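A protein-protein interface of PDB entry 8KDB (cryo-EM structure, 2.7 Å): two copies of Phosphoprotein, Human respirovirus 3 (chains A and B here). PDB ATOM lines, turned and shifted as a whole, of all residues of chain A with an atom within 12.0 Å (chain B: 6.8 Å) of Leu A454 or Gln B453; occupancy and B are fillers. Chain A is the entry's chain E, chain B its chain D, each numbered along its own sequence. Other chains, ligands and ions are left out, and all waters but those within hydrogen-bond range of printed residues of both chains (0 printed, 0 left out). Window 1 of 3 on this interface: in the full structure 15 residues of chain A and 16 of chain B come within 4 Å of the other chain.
The side-chain amide oxygen of Gln A450 lies close to the backbone carbonyl oxygen of Leu A446 (2.6 Å).
The backbone carbonyl oxygen (O) of Ser A455 sits at hydrogen-bond distance from the side-chain hydroxyl (OG1) of Thr A458, 2.5 Å away.
The side-chain amide oxygen (OE1) of Gln A450 lies close to the backbone NH (N) of Ile A447 (3.5 Å).
OG1 of Thr A458 sits close to O of Leu A454, 3.4 Å away.
Among the printed residues, pairs that only touch across the chains: Gln A450 with Gln B450 (3.8 Å), Leu A454 with Gln B450 (3.4 Å), Leu A454 with Gln B453 (3.6 Å), Ile A457 with Ile B457 (3.6 Å), Thr A458 with Gln B453 (3.98 Å), Thr A458 with Ile B457 (3.6 Å) and Ile A461 with Ile B457 (3.9 Å).
Glu A452 touches none of the printed residues of chain B.
Of the printed residues of chain B, Leu A454 touches Gln B450 and Gln B453.
Of the printed residues of chain B, Ile A457 touches Ile B457 (3.6 Å).
Of the printed residues of chain B, Thr A458 touches Gln B453 (3.98 Å) and Ile B457 (3.6 Å).
No residue of chain A comes within 4 Å of Asn B449.
Of chain A, only Gln A450 (3.8 Å) and Leu A454 (3.4 Å) come within 4 Å of Gln B450.
No residue of chain A comes within 4 Å of Glu B452.
Printed residues of chain A within 4 Å of Gln B453: Leu A454 and Thr A458.
Leu B454 touches none of the printed residues of chain A.
No residue of chain A comes within 4 Å of Ser B455.
Of chain A, only Ile A457 (3.6 Å), Thr A458 (3.6 Å) and Ile A461 (3.9 Å) come within 4 Å of Ile B457.
Thr B458 touches none of the printed residues of chain A.
The nearest residue of chain B that does not touch Leu A454 is Leu B454 (4.2 Å).
The nearest residue of chain A that does not touch Gln B453 is Ser A455 (5.5 Å).
The nearest printed residue of chain B that does not touch Ile A461 is Leu B456 (6.3 Å).
Hydrophobic or aromatic side chains of chain A that line the printed part of chain B: Leu A454, Ile A457 and Ile A461.
Hydrophobic or aromatic side chains of chain B within 4 Å of the printed part of chain A: Ile B457.
Among the printed residues, 7 pairs touch across the chains.
Leu A454 touches Gln B453, but with the chains exchanged Gln A453 does not touch Leu B454 (8.3 Å).
Ile B457 touches its own counterpart, Ile A457.
Thr A458 touches Gln B453, but with the chains exchanged Gln A453 does not touch Thr B458 (12.1 Å).
Thr A458 touches Ile B457, but with the chains exchanged Ile A457 does not touch Thr B458 (7.9 Å).
Of the 7 pairs that touch across the chains among the printed residues, 2 have their exchanged pair printed and touching as well.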
ATOM      1  N   ARG A 444      -8.823   2.347 -26.310  1.00  0.00           N
ATOM      2  CA  ARG A 444      -9.443   1.429 -25.358  1.00  0.00           C
ATOM      3  C   ARG A 444      -8.949   1.690 -23.940  1.00  0.00           C
ATOM      4  O   ARG A 444      -9.743   1.713 -22.989  1.00  0.00           O
ATOM      5  CB  ARG A 444      -9.163  -0.015 -25.772  1.00  0.00           C
ATOM      6  CG  ARG A 444      -9.965  -1.053 -25.011  1.00  0.00           C
ATOM      7  CD  ARG A 444      -9.615  -2.459 -25.471  1.00  0.00           C
ATOM      8  NE  ARG A 444      -9.944  -2.676 -26.874  1.00  0.00           N
ATOM      9  CZ  ARG A 444     -11.145  -3.018 -27.319  1.00  0.00           C
ATOM     10  NH1 ARG A 444     -12.164  -3.193 -26.493  1.00  0.00           N
ATOM     11  NH2 ARG A 444     -11.329  -3.191 -28.624  1.00  0.00           N
ATOM     12  N   ARG A 445      -7.639   1.898 -23.781  1.00  0.00           N
ATOM     13  CA  ARG A 445      -7.091   2.193 -22.460  1.00  0.00           C
ATOM     14  C   ARG A 445      -7.653   3.498 -21.908  1.00  0.00           C
ATOM     15  O   ARG A 445      -8.014   3.579 -20.726  1.00  0.00           O
ATOM     16  CB  ARG A 445      -5.565   2.253 -22.529  1.00  0.00           C
ATOM     17  CG  ARG A 445      -4.907   0.917 -22.838  1.00  0.00           C
ATOM     18  CD  ARG A 445      -3.418   0.948 -22.535  1.00  0.00           C
ATOM     19  NE  ARG A 445      -3.150   1.228 -21.129  1.00  0.00           N
ATOM     20  CZ  ARG A 445      -1.983   1.020 -20.534  1.00  0.00           C
ATOM     21  NH1 ARG A 445      -0.947   0.531 -21.195  1.00  0.00           N
ATOM     22  NH2 ARG A 445      -1.853   1.311 -19.242  1.00  0.00           N
ATOM     23  N   LEU A 446      -7.744   4.529 -22.753  1.00  0.00           N
ATOM     24  CA  LEU A 446      -8.297   5.802 -22.300  1.00  0.00           C
ATOM     25  C   LEU A 446      -9.748   5.647 -21.859  1.00  0.00           C
ATOM     26  O   LEU A 446     -10.152   6.174 -20.815  1.00  0.00           O
ATOM     27  CB  LEU A 446      -8.178   6.850 -23.407  1.00  0.00           C
ATOM     28  CG  LEU A 446      -6.760   7.260 -23.807  1.00  0.00           C
ATOM     29  CD1 LEU A 446      -6.793   8.207 -24.997  1.00  0.00           C
ATOM     30  CD2 LEU A 446      -6.028   7.889 -22.632  1.00  0.00           C
ATOM     31  N   ILE A 447     -10.545   4.916 -22.643  1.00  0.00           N
ATOM     32  CA  ILE A 447     -11.957   4.744 -22.310  1.00  0.00           C
ATOM     33  C   ILE A 447     -12.107   3.965 -21.010  1.00  0.00           C
ATOM     34  O   ILE A 447     -12.993   4.253 -20.195  1.00  0.00           O
ATOM     35  CB  ILE A 447     -12.706   4.070 -23.474  1.00  0.00           C
ATOM     36  CG1 ILE A 447     -12.695   4.973 -24.709  1.00  0.00           C
ATOM     37  CG2 ILE A 447     -14.140   3.761 -23.082  1.00  0.00           C
ATOM     38  CD1 ILE A 447     -13.108   6.398 -24.427  1.00  0.00           C
ATOM     39  N   GLU A 448     -11.241   2.974 -20.784  1.00  0.00           N
ATOM     40  CA  GLU A 448     -11.274   2.261 -19.510  1.00  0.00           C
ATOM     41  C   GLU A 448     -10.916   3.187 -18.351  1.00  0.00           C
ATOM     42  O   GLU A 448     -11.489   3.083 -17.257  1.00  0.00           O
ATOM     43  CB  GLU A 448     -10.334   1.058 -19.555  1.00  0.00           C
ATOM     44  CG  GLU A 448     -10.291   0.258 -18.264  1.00  0.00           C
ATOM     45  CD  GLU A 448     -10.244  -1.237 -18.508  1.00  0.00           C
ATOM     46  OE1 GLU A 448      -9.731  -1.653 -19.568  1.00  0.00           O
ATOM     47  OE2 GLU A 448     -10.722  -1.996 -17.639  1.00  0.00           O
ATOM     48  N   ASN A 449      -9.964   4.098 -18.570  1.00  0.00           N
ATOM     49  CA  ASN A 449      -9.634   5.084 -17.545  1.00  0.00           C
ATOM     50  C   ASN A 449     -10.843   5.953 -17.208  1.00  0.00           C
ATOM     51  O   ASN A 449     -11.148   6.195 -16.030  1.00  0.00           O
ATOM     52  CB  ASN A 449      -8.464   5.950 -18.008  1.00  0.00           C
ATOM     53  CG  ASN A 449      -7.150   5.202 -18.003  1.00  0.00           C
ATOM     54  OD1 ASN A 449      -7.096   4.025 -17.650  1.00  0.00           O
ATOM     55  ND2 ASN A 449      -6.080   5.882 -18.396  1.00  0.00           N
ATOM     56  N   GLN A 450     -11.548   6.434 -18.237  1.00  0.00           N
ATOM     57  CA  GLN A 450     -12.749   7.225 -17.972  1.00  0.00           C
ATOM     58  C   GLN A 450     -13.818   6.394 -17.274  1.00  0.00           C
ATOM     59  O   GLN A 450     -14.575   6.920 -16.454  1.00  0.00           O
ATOM     60  CB  GLN A 450     -13.315   7.857 -19.248  1.00  0.00           C
ATOM     61  CG  GLN A 450     -12.601   9.134 -19.689  1.00  0.00           C
ATOM     62  CD  GLN A 450     -11.616   8.925 -20.813  1.00  0.00           C
ATOM     63  OE1 GLN A 450     -11.768   8.015 -21.623  1.00  0.00           O
ATOM     64  NE2 GLN A 450     -10.588   9.763 -20.861  1.00  0.00           N
ATOM     65  N   ARG A 451     -13.899   5.097 -17.581  1.00  0.00           N
ATOM     66  CA  ARG A 451     -14.854   4.238 -16.883  1.00  0.00           C
ATOM     67  C   ARG A 451     -14.527   4.143 -15.397  1.00  0.00           C
ATOM     68  O   ARG A 451     -15.426   4.181 -14.547  1.00  0.00           O
ATOM     69  CB  ARG A 451     -14.873   2.847 -17.518  1.00  0.00           C
ATOM     70  CG  ARG A 451     -16.149   2.055 -17.253  1.00  0.00           C
ATOM     71  CD  ARG A 451     -16.046   1.221 -15.986  1.00  0.00           C
ATOM     72  NE  ARG A 451     -14.862   0.370 -15.982  1.00  0.00           N
ATOM     73  CZ  ARG A 451     -14.782  -0.805 -16.590  1.00  0.00           C
ATOM     74  NH1 ARG A 451     -15.806  -1.309 -17.259  1.00  0.00           N
ATOM     75  NH2 ARG A 451     -13.646  -1.494 -16.523  1.00  0.00           N
ATOM     76  N   GLU A 452     -13.242   4.004 -15.067  1.00  0.00           N
ATOM     77  CA  GLU A 452     -12.838   3.991 -13.662  1.00  0.00           C
ATOM     78  C   GLU A 452     -13.190   5.308 -12.977  1.00  0.00           C
ATOM     79  O   GLU A 452     -13.676   5.324 -11.834  1.00  0.00           O
ATOM     80  CB  GLU A 452     -11.340   3.708 -13.556  1.00  0.00           C
ATOM     81  CG  GLU A 452     -10.780   3.796 -12.146  1.00  0.00           C
ATOM     82  CD  GLU A 452      -9.268   3.901 -12.128  1.00  0.00           C
ATOM     83  OE1 GLU A 452      -8.685   4.268 -13.170  1.00  0.00           O
ATOM     84  OE2 GLU A 452      -8.663   3.615 -11.074  1.00  0.00           O
ATOM     85  N   GLN A 453     -12.954   6.426 -13.669  1.00  0.00           N
ATOM     86  CA  GLN A 453     -13.318   7.724 -13.108  1.00  0.00           C
ATOM     87  C   GLN A 453     -14.825   7.827 -12.887  1.00  0.00           C
ATOM     88  O   GLN A 453     -15.274   8.381 -11.876  1.00  0.00           O
ATOM     89  CB  GLN A 453     -12.823   8.846 -14.018  1.00  0.00           C
ATOM     90  CG  GLN A 453     -12.519  10.137 -13.284  1.00  0.00           C
ATOM     91  CD  GLN A 453     -11.597  11.045 -14.067  1.00  0.00           C
ATOM     92  OE1 GLN A 453     -11.445  10.900 -15.281  1.00  0.00           O
ATOM     93  NE2 GLN A 453     -10.969  11.988 -13.376  1.00  0.00           N
ATOM     94  N   LEU A 454     -15.619   7.298 -13.822  1.00  0.00           N
ATOM     95  CA  LEU A 454     -17.067   7.256 -13.633  1.00  0.00           C
ATOM     96  C   LEU A 454     -17.452   6.436 -12.414  1.00  0.00           C
ATOM     97  O   LEU A 454     -18.375   6.809 -11.690  1.00  0.00           O
ATOM     98  CB  LEU A 454     -17.765   6.673 -14.859  1.00  0.00           C
ATOM     99  CG  LEU A 454     -17.613   7.294 -16.239  1.00  0.00           C
ATOM    100  CD1 LEU A 454     -18.597   6.615 -17.156  1.00  0.00           C
ATOM    101  CD2 LEU A 454     -17.868   8.784 -16.186  1.00  0.00           C
ATOM    102  N   SER A 455     -16.790   5.299 -12.196  1.00  0.00           N
ATOM    103  CA  SER A 455     -17.099   4.487 -11.022  1.00  0.00           C
ATOM    104  C   SER A 455     -16.834   5.269  -9.740  1.00  0.00           C
ATOM    105  O   SER A 455     -17.648   5.259  -8.803  1.00  0.00           O
ATOM    106  CB  SER A 455     -16.283   3.195 -11.048  1.00  0.00           C
ATOM    107  OG  SER A 455     -14.932   3.442 -10.700  1.00  0.00           O
ATOM    108  N   LEU A 456     -15.699   5.972  -9.692  1.00  0.00           N
ATOM    109  CA  LEU A 456     -15.406   6.806  -8.527  1.00  0.00           C
ATOM    110  C   LEU A 456     -16.460   7.894  -8.346  1.00  0.00           C
ATOM    111  O   LEU A 456     -16.900   8.171  -7.219  1.00  0.00           O
ATOM    112  CB  LEU A 456     -14.016   7.427  -8.662  1.00  0.00           C
ATOM    113  CG  LEU A 456     -13.560   8.276  -7.475  1.00  0.00           C
ATOM    114  CD1 LEU A 456     -13.458   7.424  -6.220  1.00  0.00           C
ATOM    115  CD2 LEU A 456     -12.235   8.958  -7.777  1.00  0.00           C
ATOM    116  N   ILE A 457     -16.880   8.521  -9.447  1.00  0.00           N
ATOM    117  CA  ILE A 457     -17.872   9.589  -9.370  1.00  0.00           C
ATOM    118  C   ILE A 457     -19.205   9.047  -8.868  1.00  0.00           C
ATOM    119  O   ILE A 457     -19.891   9.693  -8.071  1.00  0.00           O
ATOM    120  CB  ILE A 457     -18.012  10.283 -10.738  1.00  0.00           C
ATOM    121  CG1 ILE A 457     -16.890  11.299 -10.935  1.00  0.00           C
ATOM    122  CG2 ILE A 457     -19.349  10.991 -10.850  1.00  0.00           C
ATOM    123  CD1 ILE A 457     -16.899  11.963 -12.290  1.00  0.00           C
ATOM    124  N   THR A 458     -19.593   7.853  -9.328  1.00  0.00           N
ATOM    125  CA  THR A 458     -20.829   7.237  -8.849  1.00  0.00           C
ATOM    126  C   THR A 458     -20.760   6.946  -7.357  1.00  0.00           C
ATOM    127  O   THR A 458     -21.740   7.152  -6.632  1.00  0.00           O
ATOM    128  CB  THR A 458     -21.133   5.949  -9.617  1.00  0.00           C
ATOM    129  OG1 THR A 458     -20.074   5.004  -9.419  1.00  0.00           O
ATOM    130  CG2 THR A 458     -21.324   6.218 -11.099  1.00  0.00           C
ATOM    131  N   SER A 459     -19.614   6.451  -6.881  1.00  0.00           N
ATOM    132  CA  SER A 459     -19.473   6.197  -5.449  1.00  0.00           C
ATOM    133  C   SER A 459     -19.620   7.488  -4.650  1.00  0.00           C
ATOM    134  O   SER A 459     -20.331   7.533  -3.634  1.00  0.00           O
ATOM    135  CB  SER A 459     -18.126   5.534  -5.165  1.00  0.00           C
ATOM    136  OG  SER A 459     -17.056   6.416  -5.453  1.00  0.00           O
ATOM    137  N   LEU A 460     -18.964   8.556  -5.111  1.00  0.00           N
ATOM    138  CA  LEU A 460     -19.074   9.843  -4.426  1.00  0.00           C
ATOM    139  C   LEU A 460     -20.509  10.356  -4.437  1.00  0.00           C
ATOM    140  O   LEU A 460     -20.996  10.884  -3.430  1.00  0.00           O
ATOM    141  CB  LEU A 460     -18.136  10.861  -5.074  1.00  0.00           C
ATOM    142  CG  LEU A 460     -16.710  10.934  -4.527  1.00  0.00           C
ATOM    143  CD1 LEU A 460     -15.864  11.869  -5.373  1.00  0.00           C
ATOM    144  CD2 LEU A 460     -16.711  11.374  -3.073  1.00  0.00           C
ATOM    145  N   ILE A 461     -21.197  10.215  -5.572  1.00  0.00           N
ATOM    146  CA  ILE A 461     -22.576  10.680  -5.691  1.00  0.00           C
ATOM    147  C   ILE A 461     -23.481   9.922  -4.732  1.00  0.00           C
ATOM    148  O   ILE A 461     -24.354  10.509  -4.081  1.00  0.00           O
ATOM    149  CB  ILE A 461     -23.057  10.543  -7.148  1.00  0.00           C
ATOM    150  CG1 ILE A 461     -22.468  11.651  -8.017  1.00  0.00           C
ATOM    151  CG2 ILE A 461     -24.573  10.583  -7.220  1.00  0.00           C
ATOM    152  CD1 ILE A 461     -23.051  13.002  -7.733  1.00  0.00           C
ATOM    153  N   SER A 462     -23.301   8.602  -4.644  1.00  0.00           N
ATOM    154  CA  SER A 462     -24.115   7.808  -3.732  1.00  0.00           C
ATOM    155  C   SER A 462     -23.871   8.214  -2.283  1.00  0.00           C
ATOM    156  O   SER A 462     -24.821   8.338  -1.499  1.00  0.00           O
ATOM    157  CB  SER A 462     -23.826   6.322  -3.930  1.00  0.00           C
ATOM    158  OG  SER A 462     -24.444   5.545  -2.920  1.00  0.00           O
ATOM    159  N   ASN A 463     -22.605   8.429  -1.911  1.00  0.00           N
ATOM    160  CA  ASN A 463     -22.317   8.884  -0.552  1.00  0.00           C
ATOM    161  C   ASN A 463     -22.970  10.235  -0.274  1.00  0.00           C
ATOM    162  O   ASN A 463     -23.554  10.445   0.798  1.00  0.00           O
ATOM    163  CB  ASN A 463     -20.807   8.967  -0.329  1.00  0.00           C
ATOM    164  CG  ASN A 463     -20.161   7.604  -0.198  1.00  0.00           C
ATOM    165  OD1 ASN A 463     -20.609   6.629  -0.799  1.00  0.00           O
ATOM    166  ND2 ASN A 463     -19.101   7.529   0.597  1.00  0.00           N
ATOM    167  N   GLU B 448     -21.499   3.700 -25.182  1.00  0.00           N
ATOM    168  CA  GLU B 448     -22.859   3.597 -24.665  1.00  0.00           C
ATOM    169  C   GLU B 448     -22.881   3.197 -23.197  1.00  0.00           C
ATOM    170  O   GLU B 448     -23.748   3.658 -22.449  1.00  0.00           O
ATOM    171  CB  GLU B 448     -23.677   2.612 -25.500  1.00  0.00           C
ATOM    172  CG  GLU B 448     -23.921   3.075 -26.926  1.00  0.00           C
ATOM    173  CD  GLU B 448     -24.809   4.301 -26.994  1.00  0.00           C
ATOM    174  OE1 GLU B 448     -25.690   4.450 -26.121  1.00  0.00           O
ATOM    175  OE2 GLU B 448     -24.624   5.118 -27.920  1.00  0.00           O
ATOM    176  N   ASN B 449     -21.947   2.347 -22.762  1.00  0.00           N
ATOM    177  CA  ASN B 449     -21.839   2.064 -21.332  1.00  0.00           C
ATOM    178  C   ASN B 449     -21.507   3.330 -20.549  1.00  0.00           C
ATOM    179  O   ASN B 449     -22.085   3.589 -19.481  1.00  0.00           O
ATOM    180  CB  ASN B 449     -20.783   0.988 -21.088  1.00  0.00           C
ATOM    181  CG  ASN B 449     -20.838   0.424 -19.682  1.00  0.00           C
ATOM    182  OD1 ASN B 449     -21.720   0.769 -18.896  1.00  0.00           O
ATOM    183  ND2 ASN B 449     -19.889  -0.445 -19.357  1.00  0.00           N
ATOM    184  N   GLN B 450     -20.578   4.134 -21.069  1.00  0.00           N
ATOM    185  CA  GLN B 450     -20.231   5.392 -20.416  1.00  0.00           C
ATOM    186  C   GLN B 450     -21.427   6.339 -20.371  1.00  0.00           C
ATOM    187  O   GLN B 450     -21.668   7.010 -19.359  1.00  0.00           O
ATOM    188  CB  GLN B 450     -19.045   6.031 -21.139  1.00  0.00           C
ATOM    189  CG  GLN B 450     -18.518   7.294 -20.499  1.00  0.00           C
ATOM    190  CD  GLN B 450     -17.270   7.810 -21.177  1.00  0.00           C
ATOM    191  OE1 GLN B 450     -16.811   7.249 -22.170  1.00  0.00           O
ATOM    192  NE2 GLN B 450     -16.696   8.872 -20.624  1.00  0.00           N
ATOM    193  N   ARG B 451     -22.196   6.389 -21.460  1.00  0.00           N
ATOM    194  CA  ARG B 451     -23.399   7.214 -21.497  1.00  0.00           C
ATOM    195  C   ARG B 451     -24.426   6.737 -20.479  1.00  0.00           C
ATOM    196  O   ARG B 451     -25.098   7.552 -19.836  1.00  0.00           O
ATOM    197  CB  ARG B 451     -23.992   7.202 -22.906  1.00  0.00           C
ATOM    198  CG  ARG B 451     -25.108   8.209 -23.144  1.00  0.00           C
ATOM    199  CD  ARG B 451     -26.475   7.562 -22.969  1.00  0.00           C
ATOM    200  NE  ARG B 451     -26.624   6.369 -23.795  1.00  0.00           N
ATOM    201  CZ  ARG B 451     -27.498   5.401 -23.563  1.00  0.00           C
ATOM    202  NH1 ARG B 451     -28.328   5.450 -22.533  1.00  0.00           N
ATOM    203  NH2 ARG B 451     -27.540   4.353 -24.381  1.00  0.00           N
ATOM    204  N   GLU B 452     -24.580   5.421 -20.334  1.00  0.00           N
ATOM    205  CA  GLU B 452     -25.509   4.886 -19.345  1.00  0.00           C
ATOM    206  C   GLU B 452     -25.094   5.280 -17.935  1.00  0.00           C
ATOM    207  O   GLU B 452     -25.935   5.673 -17.117  1.00  0.00           O
ATOM    208  CB  GLU B 452     -25.596   3.366 -19.475  1.00  0.00           C
ATOM    209  CG  GLU B 452     -26.575   2.715 -18.513  1.00  0.00           C
ATOM    210  CD  GLU B 452     -28.013   3.120 -18.775  1.00  0.00           C
ATOM    211  OE1 GLU B 452     -28.332   3.480 -19.928  1.00  0.00           O
ATOM    212  OE2 GLU B 452     -28.825   3.078 -17.828  1.00  0.00           O
ATOM    213  N   GLN B 453     -23.796   5.186 -17.631  1.00  0.00           N
ATOM    214  CA  GLN B 453     -23.325   5.608 -16.314  1.00  0.00           C
ATOM    215  C   GLN B 453     -23.583   7.094 -16.081  1.00  0.00           C
ATOM    216  O   GLN B 453     -24.036   7.494 -15.000  1.00  0.00           O
ATOM    217  CB  GLN B 453     -21.838   5.292 -16.158  1.00  0.00           C
ATOM    218  CG  GLN B 453     -21.515   3.808 -16.163  1.00  0.00           C
ATOM    219  CD  GLN B 453     -22.156   3.072 -15.003  1.00  0.00           C
ATOM    220  OE1 GLN B 453     -23.090   2.292 -15.188  1.00  0.00           O
ATOM    221  NE2 GLN B 453     -21.656   3.317 -13.798  1.00  0.00           N
ATOM    222  N   LEU B 454     -23.306   7.929 -17.087  1.00  0.00           N
ATOM    223  CA  LEU B 454     -23.530   9.364 -16.937  1.00  0.00           C
ATOM    224  C   LEU B 454     -25.008   9.679 -16.730  1.00  0.00           C
ATOM    225  O   LEU B 454     -25.362  10.526 -15.900  1.00  0.00           O
ATOM    226  CB  LEU B 454     -22.985  10.111 -18.153  1.00  0.00           C
ATOM    227  CG  LEU B 454     -21.490  10.429 -18.126  1.00  0.00           C
ATOM    228  CD1 LEU B 454     -21.049  11.072 -19.431  1.00  0.00           C
ATOM    229  CD2 LEU B 454     -21.159  11.322 -16.944  1.00  0.00           C
ATOM    230  N   SER B 455     -25.885   9.011 -17.482  1.00  0.00           N
ATOM    231  CA  SER B 455     -27.319   9.235 -17.327  1.00  0.00           C
ATOM    232  C   SER B 455     -27.800   8.786 -15.955  1.00  0.00           C
ATOM    233  O   SER B 455     -28.668   9.429 -15.354  1.00  0.00           O
ATOM    234  CB  SER B 455     -28.086   8.509 -18.430  1.00  0.00           C
ATOM    235  OG  SER B 455     -27.902   9.146 -19.681  1.00  0.00           O
ATOM    236  N   LEU B 456     -27.257   7.678 -15.445  1.00  0.00           N
ATOM    237  CA  LEU B 456     -27.616   7.238 -14.101  1.00  0.00           C
ATOM    238  C   LEU B 456     -27.189   8.265 -13.061  1.00  0.00           C
ATOM    239  O   LEU B 456     -27.947   8.569 -12.132  1.00  0.00           O
ATOM    240  CB  LEU B 456     -26.989   5.870 -13.819  1.00  0.00           C
ATOM    241  CG  LEU B 456     -27.348   5.100 -12.545  1.00  0.00           C
ATOM    242  CD1 LEU B 456     -27.171   3.614 -12.789  1.00  0.00           C
ATOM    243  CD2 LEU B 456     -26.490   5.528 -11.366  1.00  0.00           C
ATOM    244  N   ILE B 457     -25.983   8.819 -13.208  1.00  0.00           N
ATOM    245  CA  ILE B 457     -25.521   9.849 -12.278  1.00  0.00           C
ATOM    246  C   ILE B 457     -26.448  11.058 -12.324  1.00  0.00           C
ATOM    247  O   ILE B 457     -26.842  11.603 -11.285  1.00  0.00           O
ATOM    248  CB  ILE B 457     -24.069  10.249 -12.596  1.00  0.00           C
ATOM    249  CG1 ILE B 457     -23.130   9.062 -12.405  1.00  0.00           C
ATOM    250  CG2 ILE B 457     -23.635  11.415 -11.725  1.00  0.00           C
ATOM    251  CD1 ILE B 457     -21.744   9.306 -12.944  1.00  0.00           C
ATOM    252  N   THR B 458     -26.806  11.495 -13.534  1.00  0.00           N
ATOM    253  CA  THR B 458     -27.674  12.660 -13.674  1.00  0.00           C
ATOM    254  C   THR B 458     -29.041  12.413 -13.047  1.00  0.00           C
ATOM    255  O   THR B 458     -29.567  13.270 -12.325  1.00  0.00           O
ATOM    256  CB  THR B 458     -27.829  13.025 -15.150  1.00  0.00           C
ATOM    257  OG1 THR B 458     -26.553  13.373 -15.696  1.00  0.00           O
ATOM    258  CG2 THR B 458     -28.778  14.199 -15.310  1.00  0.00           C
